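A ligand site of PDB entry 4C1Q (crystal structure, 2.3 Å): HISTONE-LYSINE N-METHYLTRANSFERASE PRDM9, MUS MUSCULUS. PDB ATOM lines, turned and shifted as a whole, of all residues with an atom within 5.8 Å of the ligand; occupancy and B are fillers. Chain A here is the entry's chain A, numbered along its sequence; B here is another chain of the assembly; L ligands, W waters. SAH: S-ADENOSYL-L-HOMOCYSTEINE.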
ATOM      1  N   ILE A  60     -31.134 -11.405   1.894  1.00  0.00           N
ATOM      2  CA  ILE A  60     -31.533 -10.043   1.540  1.00  0.00           C
ATOM      3  C   ILE A  60     -32.365 -10.167   0.277  1.00  0.00           C
ATOM      4  O   ILE A  60     -31.923 -10.831  -0.673  1.00  0.00           O
ATOM      5  CB  ILE A  60     -30.323  -9.124   1.320  1.00  0.00           C
ATOM      6  CG1 ILE A  60     -29.479  -9.034   2.603  1.00  0.00           C
ATOM      7  CG2 ILE A  60     -30.765  -7.731   0.858  1.00  0.00           C
ATOM      8  CD1 ILE A  60     -28.102  -8.463   2.424  1.00  0.00           C
ATOM      9  N   PRO A  61     -33.574  -9.547   0.244  1.00  0.00           N
ATOM     10  CA  PRO A  61     -34.428  -9.579  -0.943  1.00  0.00           C
ATOM     11  C   PRO A  61     -33.761  -9.000  -2.184  1.00  0.00           C
ATOM     12  O   PRO A  61     -33.155  -7.917  -2.127  1.00  0.00           O
ATOM     13  CB  PRO A  61     -35.619  -8.684  -0.547  1.00  0.00           C
ATOM     14  CG  PRO A  61     -35.615  -8.636   0.940  1.00  0.00           C
ATOM     15  CD  PRO A  61     -34.163  -8.712   1.312  1.00  0.00           C
ATOM     16  N   GLU A  62     -33.853  -9.747  -3.274  1.00  0.00           N
ATOM     17  CA  GLU A  62     -33.329  -9.341  -4.573  1.00  0.00           C
ATOM     18  C   GLU A  62     -31.823  -9.034  -4.536  1.00  0.00           C
ATOM     19  O   GLU A  62     -31.341  -8.143  -5.238  1.00  0.00           O
ATOM     20  CB  GLU A  62     -34.128  -8.140  -5.098  1.00  0.00           C
ATOM     21  CG  GLU A  62     -34.007  -7.911  -6.595  1.00  0.00           C
ATOM     22  CD  GLU A  62     -34.772  -6.683  -7.055  1.00  0.00           C
ATOM     23  OE1 GLU A  62     -35.799  -6.344  -6.434  1.00  0.00           O
ATOM     24  OE2 GLU A  62     -34.340  -6.070  -8.062  1.00  0.00           O
ATOM     25  N   ALA A  63     -31.067  -9.773  -3.742  1.00  0.00           N
ATOM     26  CA  ALA A  63     -29.649  -9.535  -3.614  1.00  0.00           C
ATOM     27  C   ALA A  63     -28.815 -10.643  -4.231  1.00  0.00           C
ATOM     28  O   ALA A  63     -27.601 -10.657  -4.034  1.00  0.00           O
ATOM     29  CB  ALA A  63     -29.272  -9.315  -2.159  1.00  0.00           C
ATOM     30  N   GLY A  64     -29.431 -11.568  -4.987  1.00  0.00           N
ATOM     31  CA  GLY A  64     -28.682 -12.605  -5.673  1.00  0.00           C
ATOM     32  C   GLY A  64     -28.138 -13.666  -4.699  1.00  0.00           C
ATOM     33  O   GLY A  64     -28.797 -13.979  -3.721  1.00  0.00           O
ATOM     34  N   LEU A  65     -26.957 -14.198  -4.984  1.00  0.00           N
ATOM     35  CA  LEU A  65     -26.308 -15.206  -4.138  1.00  0.00           C
ATOM     36  C   LEU A  65     -25.600 -14.547  -2.968  1.00  0.00           C
ATOM     37  O   LEU A  65     -25.316 -13.347  -2.987  1.00  0.00           O
ATOM     38  CB  LEU A  65     -25.299 -16.039  -4.945  1.00  0.00           C
ATOM     39  CG  LEU A  65     -25.888 -16.941  -6.030  1.00  0.00           C
ATOM     40  CD1 LEU A  65     -24.763 -17.641  -6.800  1.00  0.00           C
ATOM     41  CD2 LEU A  65     -26.850 -17.971  -5.472  1.00  0.00           C
ATOM     42  N   GLY A  66     -25.328 -15.355  -1.946  1.00  0.00           N
ATOM     43  CA  GLY A  66     -24.634 -14.915  -0.751  1.00  0.00           C
ATOM     44  C   GLY A  66     -23.820 -16.046  -0.144  1.00  0.00           C
ATOM     45  O   GLY A  66     -23.823 -17.169  -0.663  1.00  0.00           O
ATOM     46  N   GLY A  97     -19.089  -3.113  -9.464  1.00  0.00           N
ATOM     47  CA  GLY A  97     -19.846  -3.477  -8.275  1.00  0.00           C
ATOM     48  C   GLY A  97     -19.165  -4.586  -7.475  1.00  0.00           C
ATOM     49  O   GLY A  97     -19.629  -4.970  -6.409  1.00  0.00           O
ATOM     50  N   TYR A  98     -18.040  -5.072  -8.017  1.00  0.00           N
ATOM     51  CA  TYR A  98     -17.239  -6.137  -7.431  1.00  0.00           C
ATOM     52  C   TYR A  98     -15.831  -5.684  -7.053  1.00  0.00           C
ATOM     53  O   TYR A  98     -14.949  -6.519  -6.821  1.00  0.00           O
ATOM     54  CB  TYR A  98     -17.169  -7.301  -8.411  1.00  0.00           C
ATOM     55  CG  TYR A  98     -18.482  -8.001  -8.571  1.00  0.00           C
ATOM     56  CD1 TYR A  98     -18.902  -8.912  -7.621  1.00  0.00           C
ATOM     57  CD2 TYR A  98     -19.327  -7.740  -9.631  1.00  0.00           C
ATOM     58  CE1 TYR A  98     -20.113  -9.549  -7.715  1.00  0.00           C
ATOM     59  CE2 TYR A  98     -20.548  -8.369  -9.756  1.00  0.00           C
ATOM     60  CZ  TYR A  98     -20.944  -9.266  -8.790  1.00  0.00           C
ATOM     61  OH  TYR A  98     -22.143  -9.920  -8.876  1.00  0.00           O
ATOM     62  N   ARG A 124     -16.244 -12.421  -3.415  1.00  0.00           N
ATOM     63  CA  ARG A 124     -17.090 -11.637  -4.312  1.00  0.00           C
ATOM     64  C   ARG A 124     -18.584 -11.852  -4.034  1.00  0.00           C
ATOM     65  O   ARG A 124     -19.413 -11.002  -4.361  1.00  0.00           O
ATOM     66  CB  ARG A 124     -16.799 -11.990  -5.777  1.00  0.00           C
ATOM     67  CG  ARG A 124     -17.561 -13.205  -6.272  1.00  0.00           C
ATOM     68  CD  ARG A 124     -17.128 -13.621  -7.647  1.00  0.00           C
ATOM     69  NE  ARG A 124     -17.507 -12.673  -8.709  1.00  0.00           N
ATOM     70  CZ  ARG A 124     -18.716 -12.580  -9.246  1.00  0.00           C
ATOM     71  NH1 ARG A 124     -19.719 -13.313  -8.802  1.00  0.00           N
ATOM     72  NH2 ARG A 124     -18.940 -11.722 -10.219  1.00  0.00           N
ATOM     73  N   TYR A 125     -18.922 -13.015  -3.454  1.00  0.00           N
ATOM     74  CA  TYR A 125     -20.315 -13.340  -3.192  1.00  0.00           C
ATOM     75  C   TYR A 125     -20.819 -12.819  -1.862  1.00  0.00           C
ATOM     76  O   TYR A 125     -21.988 -12.935  -1.575  1.00  0.00           O
ATOM     77  CB  TYR A 125     -20.541 -14.835  -3.277  1.00  0.00           C
ATOM     78  CG  TYR A 125     -20.334 -15.411  -4.647  1.00  0.00           C
ATOM     79  CD1 TYR A 125     -21.256 -15.182  -5.658  1.00  0.00           C
ATOM     80  CD2 TYR A 125     -19.214 -16.190  -4.937  1.00  0.00           C
ATOM     81  CE1 TYR A 125     -21.082 -15.723  -6.926  1.00  0.00           C
ATOM     82  CE2 TYR A 125     -19.026 -16.727  -6.209  1.00  0.00           C
ATOM     83  CZ  TYR A 125     -19.956 -16.503  -7.193  1.00  0.00           C
ATOM     84  OH  TYR A 125     -19.764 -17.028  -8.469  1.00  0.00           O
ATOM     85  N   VAL A 126     -19.940 -12.264  -1.030  1.00  0.00           N
ATOM     86  CA  VAL A 126     -20.358 -11.741   0.263  1.00  0.00           C
ATOM     87  C   VAL A 126     -21.131 -10.435   0.058  1.00  0.00           C
ATOM     88  O   VAL A 126     -20.641  -9.471  -0.555  1.00  0.00           O
ATOM     89  CB  VAL A 126     -19.171 -11.541   1.207  1.00  0.00           C
ATOM     90  CG1 VAL A 126     -19.653 -10.904   2.489  1.00  0.00           C
ATOM     91  CG2 VAL A 126     -18.501 -12.889   1.549  1.00  0.00           C
ATOM     92  N   ASN A 127     -22.345 -10.419   0.593  1.00  0.00           N
ATOM     93  CA  ASN A 127     -23.215  -9.300   0.464  1.00  0.00           C
ATOM     94  C   ASN A 127     -22.960  -8.221   1.504  1.00  0.00           C
ATOM     95  O   ASN A 127     -22.200  -8.405   2.445  1.00  0.00           O
ATOM     96  CB  ASN A 127     -24.677  -9.754   0.531  1.00  0.00           C
ATOM     97  CG  ASN A 127     -25.163 -10.336  -0.784  1.00  0.00           C
ATOM     98  OD1 ASN A 127     -25.112  -9.699  -1.822  1.00  0.00           O
ATOM     99  ND2 ASN A 127     -25.622 -11.565  -0.740  1.00  0.00           N
ATOM    100  N   CYS A 128     -23.613  -7.095   1.298  1.00  0.00           N
ATOM    101  CA  CYS A 128     -23.426  -5.919   2.130  1.00  0.00           C
ATOM    102  C   CYS A 128     -24.399  -5.855   3.272  1.00  0.00           C
ATOM    103  O   CYS A 128     -25.608  -5.975   3.068  1.00  0.00           O
ATOM    104  CB  CYS A 128     -23.660  -4.667   1.296  1.00  0.00           C
ATOM    105  SG  CYS A 128     -23.077  -3.144   2.043  1.00  0.00           S
ATOM    106  N   ALA A 129     -23.902  -5.624   4.485  1.00  0.00           N
ATOM    107  CA  ALA A 129     -24.795  -5.425   5.612  1.00  0.00           C
ATOM    108  C   ALA A 129     -25.559  -4.116   5.446  1.00  0.00           C
ATOM    109  O   ALA A 129     -25.018  -3.148   4.913  1.00  0.00           O
ATOM    110  CB  ALA A 129     -24.032  -5.413   6.920  1.00  0.00           C
ATOM    111  N   ARG A 130     -26.823  -4.107   5.871  1.00  0.00           N
ATOM    112  CA  ARG A 130     -27.661  -2.905   5.787  1.00  0.00           C
ATOM    113  C   ARG A 130     -27.787  -2.232   7.149  1.00  0.00           C
ATOM    114  O   ARG A 130     -28.180  -1.079   7.242  1.00  0.00           O
ATOM    115  CB  ARG A 130     -29.061  -3.230   5.293  1.00  0.00           C
ATOM    116  CG  ARG A 130     -29.119  -3.913   3.935  1.00  0.00           C
ATOM    117  CD  ARG A 130     -30.435  -4.658   3.751  1.00  0.00           C
ATOM    118  NE  ARG A 130     -30.559  -5.786   4.687  1.00  0.00           N
ATOM    119  CZ  ARG A 130     -31.575  -6.661   4.689  1.00  0.00           C
ATOM    120  NH1 ARG A 130     -32.582  -6.543   3.830  1.00  0.00           N
ATOM    121  NH2 ARG A 130     -31.596  -7.666   5.546  1.00  0.00           N
ATOM    122  N   GLU A 134     -26.726  -6.858  11.563  1.00  0.00           N
ATOM    123  CA  GLU A 134     -26.557  -8.044  10.714  1.00  0.00           C
ATOM    124  C   GLU A 134     -25.127  -8.099  10.145  1.00  0.00           C
ATOM    125  O   GLU A 134     -24.758  -9.076   9.516  1.00  0.00           O
ATOM    126  CB  GLU A 134     -27.621  -8.109   9.580  1.00  0.00           C
ATOM    127  CG  GLU A 134     -27.505  -7.026   8.524  1.00  0.00           C
ATOM    128  CD  GLU A 134     -28.517  -7.169   7.383  1.00  0.00           C
ATOM    129  OE1 GLU A 134     -29.429  -8.027   7.451  1.00  0.00           O
ATOM    130  OE2 GLU A 134     -28.394  -6.421   6.367  1.00  0.00           O
ATOM    131  N   TYR A 164     -19.789  -2.313   2.800  1.00  0.00           N
ATOM    132  CA  TYR A 164     -19.135  -1.946   1.534  1.00  0.00           C
ATOM    133  C   TYR A 164     -18.477  -0.532   1.520  1.00  0.00           C
ATOM    134  O   TYR A 164     -17.727  -0.197   0.590  1.00  0.00           O
ATOM    135  CB  TYR A 164     -20.153  -2.028   0.364  1.00  0.00           C
ATOM    136  CG  TYR A 164     -20.557  -3.401  -0.150  1.00  0.00           C
ATOM    137  CD1 TYR A 164     -20.245  -4.578   0.532  1.00  0.00           C
ATOM    138  CD2 TYR A 164     -21.302  -3.515  -1.330  1.00  0.00           C
ATOM    139  CE1 TYR A 164     -20.640  -5.822   0.042  1.00  0.00           C
ATOM    140  CE2 TYR A 164     -21.714  -4.756  -1.824  1.00  0.00           C
ATOM    141  CZ  TYR A 164     -21.378  -5.910  -1.147  1.00  0.00           C
ATOM    142  OH  TYR A 164     -21.783  -7.144  -1.638  1.00  0.00           O
ATOM    143  N   TYR A 168     -21.131   3.150  -1.665  1.00  0.00           N
ATOM    144  CA  TYR A 168     -21.831   2.007  -2.265  1.00  0.00           C
ATOM    145  C   TYR A 168     -23.143   1.727  -1.496  1.00  0.00           C
ATOM    146  O   TYR A 168     -24.153   1.359  -2.077  1.00  0.00           O
ATOM    147  CB  TYR A 168     -20.876   0.783  -2.267  1.00  0.00           C
ATOM    148  CG  TYR A 168     -21.176  -0.353  -3.238  1.00  0.00           C
ATOM    149  CD1 TYR A 168     -22.484  -0.788  -3.477  1.00  0.00           C
ATOM    150  CD2 TYR A 168     -20.138  -1.038  -3.873  1.00  0.00           C
ATOM    151  CE1 TYR A 168     -22.749  -1.844  -4.338  1.00  0.00           C
ATOM    152  CE2 TYR A 168     -20.403  -2.094  -4.733  1.00  0.00           C
ATOM    153  CZ  TYR A 168     -21.716  -2.484  -4.959  1.00  0.00           C
ATOM    154  OH  TYR A 168     -22.018  -3.544  -5.792  1.00  0.00           O
ATOM    155  N   LEU A 172     -26.903   1.360  -2.756  1.00  0.00           N
ATOM    156  CA  LEU A 172     -27.803   0.235  -2.435  1.00  0.00           C
ATOM    157  C   LEU A 172     -29.096   0.661  -1.702  1.00  0.00           C
ATOM    158  O   LEU A 172     -29.948  -0.184  -1.425  1.00  0.00           O
ATOM    159  CB  LEU A 172     -27.066  -0.836  -1.615  1.00  0.00           C
ATOM    160  CG  LEU A 172     -25.980  -1.685  -2.288  1.00  0.00           C
ATOM    161  CD1 LEU A 172     -25.249  -2.541  -1.262  1.00  0.00           C
ATOM    162  CD2 LEU A 172     -26.575  -2.545  -3.389  1.00  0.00           C
ATOM    163  N   ILE A 174     -29.309   2.093   1.431  1.00  0.00           N
ATOM    164  CA  ILE A 174     -29.276   1.690   2.833  1.00  0.00           C
ATOM    165  C   ILE A 174     -29.479   2.881   3.785  1.00  0.00           C
ATOM    166  O   ILE A 174     -28.751   3.876   3.724  1.00  0.00           O
ATOM    167  CB  ILE A 174     -27.988   0.860   3.138  1.00  0.00           C
ATOM    168  CG1 ILE A 174     -28.132  -0.526   2.494  1.00  0.00           C
ATOM    169  CG2 ILE A 174     -27.764   0.709   4.646  1.00  0.00           C
ATOM    170  CD1 ILE A 174     -26.828  -1.289   2.290  1.00  0.00           C
ATOM    171  N   ARG B   2     -20.323   2.370  -7.375  1.00  0.00           N
ATOM    172  CA  ARG B   2     -20.341   1.003  -6.824  1.00  0.00           C
ATOM    173  C   ARG B   2     -18.909   0.498  -6.649  1.00  0.00           C
ATOM    174  O   ARG B   2     -18.514  -0.548  -7.210  1.00  0.00           O
ATOM    175  CB  ARG B   2     -21.147   0.070  -7.740  1.00  0.00           C
ATOM    176  CG  ARG B   2     -22.579   0.512  -7.940  1.00  0.00           C
ATOM    177  CD  ARG B   2     -23.500  -0.647  -8.258  1.00  0.00           C
ATOM    178  NE  ARG B   2     -24.823  -0.428  -7.664  1.00  0.00           N
ATOM    179  CZ  ARG B   2     -25.825  -1.304  -7.725  1.00  0.00           C
ATOM    180  NH1 ARG B   2     -25.676  -2.474  -8.354  1.00  0.00           N
ATOM    181  NH2 ARG B   2     -26.987  -1.019  -7.146  1.00  0.00           N
ATOM    182  N   MLY B   4     -16.327  -0.482  -3.565  1.00  0.00           N
ATOM    183  CA  MLY B   4     -16.250  -0.790  -2.143  1.00  0.00           C
ATOM    184  CB  MLY B   4     -16.277  -2.310  -1.945  1.00  0.00           C
ATOM    185  CG  MLY B   4     -17.492  -2.968  -2.576  1.00  0.00           C
ATOM    186  CD  MLY B   4     -17.364  -4.456  -2.364  1.00  0.00           C
ATOM    187  CE  MLY B   4     -18.301  -5.210  -3.288  1.00  0.00           C
ATOM    188  NZ  MLY B   4     -18.224  -6.677  -3.078  1.00  0.00           N
ATOM    189  CH1 MLY B   4     -16.986  -7.243  -3.627  1.00  0.00           C
ATOM    190  CH2 MLY B   4     -19.339  -7.341  -3.758  1.00  0.00           C
ATOM    191  C   MLY B   4     -15.021  -0.084  -1.589  1.00  0.00           C
ATOM    192  O   MLY B   4     -13.954  -0.080  -2.208  1.00  0.00           O
HETATM  193  N   SAH L   1     -25.178 -10.693  -4.699  1.00  0.00           N
HETATM  194  CA  SAH L   1     -24.044 -10.655  -5.628  1.00  0.00           C
HETATM  195  CB  SAH L   1     -22.725 -10.733  -4.832  1.00  0.00           C
HETATM  196  CG  SAH L   1     -22.342  -9.399  -4.175  1.00  0.00           C
HETATM  197  SD  SAH L   1     -21.978  -8.239  -5.443  1.00  0.00           S
HETATM  198  C   SAH L   1     -24.110 -11.766  -6.655  1.00  0.00           C
HETATM  199  O   SAH L   1     -23.125 -12.074  -7.356  1.00  0.00           O
HETATM  200  OXT SAH L   1     -25.157 -12.390  -6.854  1.00  0.00           O
HETATM  201  C5' SAH L   1     -22.875  -6.774  -5.032  1.00  0.00           C
HETATM  202  C4' SAH L   1     -24.247  -6.874  -5.665  1.00  0.00           C
HETATM  203  O4' SAH L   1     -25.073  -7.737  -4.881  1.00  0.00           O
HETATM  204  C3' SAH L   1     -24.940  -5.539  -5.712  1.00  0.00           C
HETATM  205  O3' SAH L   1     -24.824  -5.015  -7.019  1.00  0.00           O
HETATM  206  C2' SAH L   1     -26.373  -5.876  -5.359  1.00  0.00           C
HETATM  207  O2' SAH L   1     -27.110  -6.265  -6.504  1.00  0.00           O
HETATM  208  C1' SAH L   1     -26.315  -7.120  -4.509  1.00  0.00           C
HETATM  209  N9  SAH L   1     -26.362  -6.731  -3.080  1.00  0.00           N
HETATM  210  C8  SAH L   1     -25.371  -6.830  -2.155  1.00  0.00           C
HETATM  211  N7  SAH L   1     -25.776  -6.351  -0.962  1.00  0.00           N
HETATM  212  C5  SAH L   1     -27.052  -5.921  -1.118  1.00  0.00           C
HETATM  213  C6  SAH L   1     -28.115  -5.296  -0.286  1.00  0.00           C
HETATM  214  N6  SAH L   1     -27.861  -5.029   0.998  1.00  0.00           N
HETATM  215  N1  SAH L   1     -29.336  -4.998  -0.820  1.00  0.00           N
HETATM  216  C2  SAH L   1     -29.604  -5.259  -2.122  1.00  0.00           C
HETATM  217  N3  SAH L   1     -28.690  -5.812  -2.949  1.00  0.00           N
HETATM  218  C4  SAH L   1     -27.433  -6.161  -2.518  1.00  0.00           C
HETATM  219  O   HOH W   1     -26.985  -9.608  -6.722  1.00  0.00           O
HETATM  220  O   HOH W   2     -30.666  -3.234   0.961  1.00  0.00           O
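Ile 60 touches the ligand.
CA of Gly 64 touches OXT of the ligand (3.7 Å).
O of Gly 97 touches C5' of the ligand, at 3.96 Å.
Tyr 125 touches the ligand (CA to CB, 3.9 Å).
CG of Arg 130 touches N6 of the ligand, 3.4 Å away.
OH of Tyr 164 touches CG of the ligand, 3.4 Å away.
CD2 of Leu 172 touches C4 of the ligand (3.8 Å).
MLY 4 of chain B touches the ligand.
Of the 23 residues printed, 16 come within 4 Å of the ligand.
The nearest printed residue that does not touch the ligand is Val 126 (4.0004 Å).
Water W1 lies within hydrogen-bond range of N of the ligand and O of Ala 63.
O of Ala 63 lies close to OD1 of Asn 127 (3.5 Å).
The side-chain amide nitrogen of Asn 127 lies within hydrogen-bond range of the backbone carbonyl oxygen of Leu 65 (2.9 Å).
O of Arg 2 of chain B sits close to N of Gly 97 (3.5 Å).
The side-chain hydroxyl (OH) of Tyr 164 is in hydrogen-bond range of the backbone NH (N) of Cys 128 (3.5 Å).
NE of Arg 130 is in salt-bridge range of OE2 of Glu 134.
OH of Tyr 168 lies within hydrogen-bond range of O of Gly 97, at 2.8 Å.
O of Val 126 lies within hydrogen-bond range of OH of Tyr 164.
The backbone carbonyl oxygen (O) of Ala 63 is in hydrogen-bond range of a nitrogen (N) of the ligand (2.5 Å).
The side-chain hydroxyl of Tyr 98 sits at hydrogen-bond distance from an oxygen (O) of the ligand (2.8 Å).
A nitrogen (N) of the ligand sits close to the side-chain amide oxygen (OD1) of Asn 127, at 3.0 Å.
O3' of the ligand sits at hydrogen-bond distance from NH1 of Arg 2 of chain B.
N of Leu 65 lies within hydrogen-bond range of OXT of the ligand (3.2 Å).
A nitrogen (N) of the ligand lies within hydrogen-bond range of the backbone carbonyl oxygen (O) of Leu 65, at 3.2 Å.
N of Cys 128 is in hydrogen-bond range of N7 of the ligand (3.2 Å).
A nitrogen (N6) of the ligand sits at hydrogen-bond distance from the backbone carbonyl oxygen (O) of Cys 128 (3.2 Å).
The guanidinium group (NH1) of Arg 124 is in salt-bridge range of an oxygen (O) of the ligand (3.9 Å).
OH of Tyr 168 is in hydrogen-bond range of O3' of the ligand (3.4 Å).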
